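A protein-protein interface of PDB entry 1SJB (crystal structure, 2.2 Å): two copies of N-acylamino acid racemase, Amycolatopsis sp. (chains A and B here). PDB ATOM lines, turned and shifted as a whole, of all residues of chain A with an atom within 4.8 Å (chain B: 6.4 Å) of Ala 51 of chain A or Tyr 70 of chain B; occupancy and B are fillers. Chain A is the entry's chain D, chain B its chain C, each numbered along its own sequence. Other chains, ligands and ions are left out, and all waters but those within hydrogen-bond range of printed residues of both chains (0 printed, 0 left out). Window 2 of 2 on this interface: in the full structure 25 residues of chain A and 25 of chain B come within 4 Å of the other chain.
O of Ala 51 of chain A is in hydrogen-bond range of OH of Tyr 70 of chain B, 2.9 Å away. The side-chain hydroxyl of Tyr 59 of chain A sits at hydrogen-bond distance from a ring nitrogen (ND1) of His 65 of chain B (2.8 Å). N of Val 66 of chain B lies within hydrogen-bond range of OH of Tyr 59 of chain A, at 3.4 Å.
O of Val 66 of chain B sits at hydrogen-bond distance from N of Leu 71 of chain B (2.9 Å). N of Ala 51 of chain A lies close to ND2 of Asn 60 of chain A (3.5 Å).
Of chain B, only Tyr 70 (2.9 Å) comes within 4 Å of Ala 51 of chain A. Printed residues of chain B within 4 Å of Gly 52 of chain A: Tyr 70. Printed residues of chain B within 4 Å of Pro 53 of chain A: Phe 93. Printed residues of chain B within 4 Å of Tyr 59 of chain A: His 65 (2.8 Å), Val 66 (3.4 Å) and Tyr 70 (3.3 Å). Of the printed residues of chain A, His 65 of chain B touches Tyr 59 (2.8 Å). Of the printed residues of chain A, Tyr 70 of chain B touches Ala 51, Gly 52 and Tyr 59. Of the printed residues of chain A, Phe 93 of chain B touches Pro 53 (3.4 Å). The nearest printed residue of chain A that does not touch Tyr 70 of chain B is Pro 53 of chain A (4.01 Å).
No position is printed for both chains. Of the 6 pairs that touch across the chains among the printed residues, none has its exchanged pair printed and touching as well.
Among the printed residues, pairs that only touch across the chains: Tyr 59 of chain A with Tyr 70 of chain B (3.3 Å), Pro 53 of chain A with Phe 93 of chain B (3.4 Å) and Gly 52 of chain A with Tyr 70 of chain B (3.7 Å).
Of the 8 printed residues of chain A, 4 touch a printed residue of chain B. Among the printed residues, no Asp or Glu carboxylate lies within 4 Å of a Lys or Arg side-chain nitrogen of the other chain.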
ATOM      1  N   GLU A  30     -13.601 -39.149   4.500  1.00  0.00           N
ATOM      2  CA  GLU A  30     -12.239 -39.042   4.968  1.00  0.00           C
ATOM      3  C   GLU A  30     -12.270 -38.405   6.340  1.00  0.00           C
ATOM      4  O   GLU A  30     -12.586 -37.221   6.451  1.00  0.00           O
ATOM      5  CB  GLU A  30     -11.382 -38.247   3.991  1.00  0.00           C
ATOM      6  CG  GLU A  30     -10.017 -37.855   4.558  1.00  0.00           C
ATOM      7  CD  GLU A  30      -9.264 -37.019   3.572  1.00  0.00           C
ATOM      8  OE1 GLU A  30      -8.712 -37.494   2.591  1.00  0.00           O
ATOM      9  OE2 GLU A  30      -9.317 -35.726   3.848  1.00  0.00           O
ATOM     10  N   THR A  49     -15.214 -33.272  10.968  1.00  0.00           N
ATOM     11  CA  THR A  49     -14.895 -32.483   9.791  1.00  0.00           C
ATOM     12  C   THR A  49     -14.910 -33.296   8.502  1.00  0.00           C
ATOM     13  O   THR A  49     -14.936 -34.534   8.437  1.00  0.00           O
ATOM     14  CB  THR A  49     -13.565 -31.779   9.923  1.00  0.00           C
ATOM     15  OG1 THR A  49     -12.623 -32.781  10.200  1.00  0.00           O
ATOM     16  CG2 THR A  49     -13.647 -30.775  11.073  1.00  0.00           C
ATOM     17  N   MET A  50     -14.869 -32.604   7.430  1.00  0.00           N
ATOM     18  CA  MET A  50     -14.820 -33.362   6.244  1.00  0.00           C
ATOM     19  C   MET A  50     -13.655 -32.878   5.422  1.00  0.00           C
ATOM     20  O   MET A  50     -12.795 -32.078   5.896  1.00  0.00           O
ATOM     21  CB  MET A  50     -16.172 -33.446   5.529  1.00  0.00           C
ATOM     22  CG  MET A  50     -17.227 -34.074   6.433  1.00  0.00           C
ATOM     23  SD  MET A  50     -18.564 -34.904   5.522  1.00  0.00           S
ATOM     24  CE  MET A  50     -19.291 -35.971   6.798  1.00  0.00           C
ATOM     25  N   ALA A  51     -13.606 -33.394   4.222  1.00  0.00           N
ATOM     26  CA  ALA A  51     -12.544 -33.023   3.323  1.00  0.00           C
ATOM     27  C   ALA A  51     -12.419 -31.519   3.217  1.00  0.00           C
ATOM     28  O   ALA A  51     -11.354 -30.960   3.502  1.00  0.00           O
ATOM     29  CB  ALA A  51     -12.813 -33.663   1.990  1.00  0.00           C
ATOM     30  N   GLY A  52     -13.541 -30.872   2.840  1.00  0.00           N
ATOM     31  CA  GLY A  52     -13.563 -29.404   2.719  1.00  0.00           C
ATOM     32  C   GLY A  52     -14.548 -28.700   3.661  1.00  0.00           C
ATOM     33  O   GLY A  52     -15.383 -29.365   4.310  1.00  0.00           O
ATOM     34  N   PRO A  53     -14.428 -27.346   3.715  1.00  0.00           N
ATOM     35  CA  PRO A  53     -15.301 -26.468   4.528  1.00  0.00           C
ATOM     36  C   PRO A  53     -16.681 -26.201   3.836  1.00  0.00           C
ATOM     37  O   PRO A  53     -16.924 -25.145   3.265  1.00  0.00           O
ATOM     38  CB  PRO A  53     -14.506 -25.153   4.713  1.00  0.00           C
ATOM     39  CG  PRO A  53     -13.270 -25.211   3.810  1.00  0.00           C
ATOM     40  CD  PRO A  53     -13.187 -26.638   3.266  1.00  0.00           C
ATOM     41  N   TYR A  59     -12.534 -28.160   8.360  1.00  0.00           N
ATOM     42  CA  TYR A  59     -12.219 -29.235   7.462  1.00  0.00           C
ATOM     43  C   TYR A  59     -11.069 -30.079   7.987  1.00  0.00           C
ATOM     44  O   TYR A  59     -10.230 -29.629   8.791  1.00  0.00           O
ATOM     45  CB  TYR A  59     -12.078 -28.767   6.010  1.00  0.00           C
ATOM     46  CG  TYR A  59     -10.937 -27.806   5.787  1.00  0.00           C
ATOM     47  CD1 TYR A  59     -10.927 -26.552   6.393  1.00  0.00           C
ATOM     48  CD2 TYR A  59      -9.874 -28.110   4.930  1.00  0.00           C
ATOM     49  CE1 TYR A  59      -9.904 -25.628   6.172  1.00  0.00           C
ATOM     50  CE2 TYR A  59      -8.841 -27.189   4.698  1.00  0.00           C
ATOM     51  CZ  TYR A  59      -8.846 -25.933   5.320  1.00  0.00           C
ATOM     52  OH  TYR A  59      -7.837 -24.976   5.146  1.00  0.00           O
ATOM     53  N   ASN A  60     -11.042 -31.330   7.581  1.00  0.00           N
ATOM     54  CA  ASN A  60      -9.993 -32.212   8.075  1.00  0.00           C
ATOM     55  C   ASN A  60      -8.572 -31.638   8.213  1.00  0.00           C
ATOM     56  O   ASN A  60      -7.954 -31.684   9.285  1.00  0.00           O
ATOM     57  CB  ASN A  60      -9.962 -33.496   7.277  1.00  0.00           C
ATOM     58  CG  ASN A  60     -11.137 -34.397   7.553  1.00  0.00           C
ATOM     59  OD1 ASN A  60     -11.639 -34.479   8.693  1.00  0.00           O
ATOM     60  ND2 ASN A  60     -11.575 -35.103   6.503  1.00  0.00           N
ATOM     61  N   HIS B  65      -3.590 -22.093   4.009  1.00  0.00           N
ATOM     62  CA  HIS B  65      -4.131 -23.349   3.563  1.00  0.00           C
ATOM     63  C   HIS B  65      -5.415 -23.255   2.798  1.00  0.00           C
ATOM     64  O   HIS B  65      -5.578 -23.874   1.743  1.00  0.00           O
ATOM     65  CB  HIS B  65      -4.207 -24.378   4.696  1.00  0.00           C
ATOM     66  CG  HIS B  65      -4.426 -25.752   4.177  1.00  0.00           C
ATOM     67  ND1 HIS B  65      -5.678 -26.183   3.791  1.00  0.00           N
ATOM     68  CD2 HIS B  65      -3.557 -26.770   3.984  1.00  0.00           C
ATOM     69  CE1 HIS B  65      -5.557 -27.448   3.400  1.00  0.00           C
ATOM     70  NE2 HIS B  65      -4.289 -27.833   3.501  1.00  0.00           N
ATOM     71  N   VAL B  66      -6.355 -22.523   3.350  1.00  0.00           N
ATOM     72  CA  VAL B  66      -7.609 -22.451   2.671  1.00  0.00           C
ATOM     73  C   VAL B  66      -7.461 -21.707   1.368  1.00  0.00           C
ATOM     74  O   VAL B  66      -8.050 -22.075   0.321  1.00  0.00           O
ATOM     75  CB  VAL B  66      -8.697 -21.908   3.577  1.00  0.00           C
ATOM     76  CG1 VAL B  66      -8.521 -20.418   3.802  1.00  0.00           C
ATOM     77  CG2 VAL B  66     -10.035 -22.220   2.951  1.00  0.00           C
ATOM     78  N   LEU B  67      -6.614 -20.668   1.435  1.00  0.00           N
ATOM     79  CA  LEU B  67      -6.341 -19.853   0.254  1.00  0.00           C
ATOM     80  C   LEU B  67      -5.764 -20.684  -0.863  1.00  0.00           C
ATOM     81  O   LEU B  67      -6.220 -20.654  -2.036  1.00  0.00           O
ATOM     82  CB  LEU B  67      -5.374 -18.709   0.567  1.00  0.00           C
ATOM     83  CG  LEU B  67      -6.061 -17.430   1.020  1.00  0.00           C
ATOM     84  CD1 LEU B  67      -5.079 -16.551   1.774  1.00  0.00           C
ATOM     85  CD2 LEU B  67      -6.595 -16.663  -0.192  1.00  0.00           C
ATOM     86  N   ARG B  68      -4.742 -21.450  -0.465  1.00  0.00           N
ATOM     87  CA  ARG B  68      -4.016 -22.315  -1.374  1.00  0.00           C
ATOM     88  C   ARG B  68      -4.875 -23.384  -1.971  1.00  0.00           C
ATOM     89  O   ARG B  68      -4.918 -23.544  -3.189  1.00  0.00           O
ATOM     90  CB  ARG B  68      -2.786 -22.965  -0.751  1.00  0.00           C
ATOM     91  CG  ARG B  68      -1.569 -22.048  -0.498  1.00  0.00           C
ATOM     92  CD  ARG B  68      -0.276 -22.835  -0.178  1.00  0.00           C
ATOM     93  NE  ARG B  68       0.061 -23.855  -1.184  1.00  0.00           N
ATOM     94  CZ  ARG B  68       1.224 -24.482  -1.248  1.00  0.00           C
ATOM     95  NH1 ARG B  68       2.195 -24.235  -0.370  1.00  0.00           N
ATOM     96  NH2 ARG B  68       1.408 -25.387  -2.212  1.00  0.00           N
ATOM     97  N   HIS B  69      -5.555 -24.125  -1.100  1.00  0.00           N
ATOM     98  CA  HIS B  69      -6.349 -25.253  -1.550  1.00  0.00           C
ATOM     99  C   HIS B  69      -7.740 -25.004  -1.983  1.00  0.00           C
ATOM    100  O   HIS B  69      -8.270 -25.768  -2.791  1.00  0.00           O
ATOM    101  CB  HIS B  69      -6.278 -26.445  -0.583  1.00  0.00           C
ATOM    102  CG  HIS B  69      -4.856 -26.796  -0.421  1.00  0.00           C
ATOM    103  ND1 HIS B  69      -4.206 -27.527  -1.392  1.00  0.00           N
ATOM    104  CD2 HIS B  69      -3.963 -26.418   0.517  1.00  0.00           C
ATOM    105  CE1 HIS B  69      -2.944 -27.611  -1.007  1.00  0.00           C
ATOM    106  NE2 HIS B  69      -2.767 -26.952   0.136  1.00  0.00           N
ATOM    107  N   TYR B  70      -8.360 -23.986  -1.426  1.00  0.00           N
ATOM    108  CA  TYR B  70      -9.734 -23.784  -1.790  1.00  0.00           C
ATOM    109  C   TYR B  70     -10.058 -22.506  -2.538  1.00  0.00           C
ATOM    110  O   TYR B  70     -10.495 -22.581  -3.672  1.00  0.00           O
ATOM    111  CB  TYR B  70     -10.659 -24.055  -0.596  1.00  0.00           C
ATOM    112  CG  TYR B  70     -10.484 -25.451  -0.026  1.00  0.00           C
ATOM    113  CD1 TYR B  70      -9.536 -25.729   0.962  1.00  0.00           C
ATOM    114  CD2 TYR B  70     -11.276 -26.501  -0.489  1.00  0.00           C
ATOM    115  CE1 TYR B  70      -9.386 -27.018   1.478  1.00  0.00           C
ATOM    116  CE2 TYR B  70     -11.139 -27.797   0.016  1.00  0.00           C
ATOM    117  CZ  TYR B  70     -10.196 -28.057   1.012  1.00  0.00           C
ATOM    118  OH  TYR B  70     -10.032 -29.338   1.514  1.00  0.00           O
ATOM    119  N   LEU B  71      -9.835 -21.346  -1.899  1.00  0.00           N
ATOM    120  CA  LEU B  71     -10.153 -20.046  -2.477  1.00  0.00           C
ATOM    121  C   LEU B  71      -9.472 -19.712  -3.786  1.00  0.00           C
ATOM    122  O   LEU B  71     -10.128 -19.495  -4.810  1.00  0.00           O
ATOM    123  CB  LEU B  71      -9.896 -18.920  -1.480  1.00  0.00           C
ATOM    124  CG  LEU B  71     -10.361 -19.294  -0.090  1.00  0.00           C
ATOM    125  CD1 LEU B  71     -10.214 -18.085   0.848  1.00  0.00           C
ATOM    126  CD2 LEU B  71     -11.811 -19.734  -0.194  1.00  0.00           C
ATOM    127  N   ILE B  72      -8.146 -19.611  -3.744  1.00  0.00           N
ATOM    128  CA  ILE B  72      -7.417 -19.221  -4.930  1.00  0.00           C
ATOM    129  C   ILE B  72      -7.780 -20.010  -6.170  1.00  0.00           C
ATOM    130  O   ILE B  72      -8.135 -19.500  -7.248  1.00  0.00           O
ATOM    131  CB  ILE B  72      -5.946 -19.109  -4.687  1.00  0.00           C
ATOM    132  CG1 ILE B  72      -5.715 -17.952  -3.725  1.00  0.00           C
ATOM    133  CG2 ILE B  72      -5.306 -18.763  -6.027  1.00  0.00           C
ATOM    134  CD1 ILE B  72      -4.236 -17.654  -3.465  1.00  0.00           C
ATOM    135  N   PRO B  73      -7.713 -21.283  -5.999  1.00  0.00           N
ATOM    136  CA  PRO B  73      -8.049 -22.159  -7.069  1.00  0.00           C
ATOM    137  C   PRO B  73      -9.430 -21.878  -7.608  1.00  0.00           C
ATOM    138  O   PRO B  73      -9.687 -21.946  -8.820  1.00  0.00           O
ATOM    139  CB  PRO B  73      -7.943 -23.563  -6.497  1.00  0.00           C
ATOM    140  CG  PRO B  73      -7.097 -23.431  -5.238  1.00  0.00           C
ATOM    141  CD  PRO B  73      -7.014 -21.963  -4.867  1.00  0.00           C
ATOM    142  N   ALA B  74     -10.304 -21.575  -6.688  1.00  0.00           N
ATOM    143  CA  ALA B  74     -11.651 -21.305  -7.050  1.00  0.00           C
ATOM    144  C   ALA B  74     -11.685 -20.148  -8.009  1.00  0.00           C
ATOM    145  O   ALA B  74     -12.463 -20.100  -8.956  1.00  0.00           O
ATOM    146  CB  ALA B  74     -12.431 -20.949  -5.807  1.00  0.00           C
ATOM    147  N   LEU B  75     -10.828 -19.185  -7.770  1.00  0.00           N
ATOM    148  CA  LEU B  75     -10.836 -18.032  -8.642  1.00  0.00           C
ATOM    149  C   LEU B  75     -10.193 -18.279  -9.979  1.00  0.00           C
ATOM    150  O   LEU B  75     -10.602 -17.748 -11.004  1.00  0.00           O
ATOM    151  CB  LEU B  75     -10.254 -16.809  -7.939  1.00  0.00           C
ATOM    152  CG  LEU B  75     -11.027 -16.502  -6.662  1.00  0.00           C
ATOM    153  CD1 LEU B  75     -10.339 -15.337  -5.984  1.00  0.00           C
ATOM    154  CD2 LEU B  75     -12.509 -16.171  -6.948  1.00  0.00           C
ATOM    155  N   LEU B  90     -16.717 -17.674  -4.136  1.00  0.00           N
ATOM    156  CA  LEU B  90     -16.124 -18.334  -3.008  1.00  0.00           C
ATOM    157  C   LEU B  90     -17.137 -18.703  -1.953  1.00  0.00           C
ATOM    158  O   LEU B  90     -16.778 -19.216  -0.903  1.00  0.00           O
ATOM    159  CB  LEU B  90     -14.985 -17.473  -2.416  1.00  0.00           C
ATOM    160  CG  LEU B  90     -13.887 -17.028  -3.395  1.00  0.00           C
ATOM    161  CD1 LEU B  90     -12.844 -16.254  -2.615  1.00  0.00           C
ATOM    162  CD2 LEU B  90     -13.187 -18.230  -4.011  1.00  0.00           C
ATOM    163  N   PHE B  93     -17.652 -22.045   0.265  1.00  0.00           N
ATOM    164  CA  PHE B  93     -16.767 -22.333   1.378  1.00  0.00           C
ATOM    165  C   PHE B  93     -17.190 -21.574   2.572  1.00  0.00           C
ATOM    166  O   PHE B  93     -17.297 -20.350   2.507  1.00  0.00           O
ATOM    167  CB  PHE B  93     -15.349 -21.892   1.006  1.00  0.00           C
ATOM    168  CG  PHE B  93     -14.945 -22.507  -0.314  1.00  0.00           C
ATOM    169  CD1 PHE B  93     -14.684 -21.691  -1.418  1.00  0.00           C
ATOM    170  CD2 PHE B  93     -14.860 -23.894  -0.452  1.00  0.00           C
ATOM    171  CE1 PHE B  93     -14.329 -22.251  -2.642  1.00  0.00           C
ATOM    172  CE2 PHE B  93     -14.512 -24.473  -1.669  1.00  0.00           C
ATOM    173  CZ  PHE B  93     -14.241 -23.641  -2.756  1.00  0.00           C
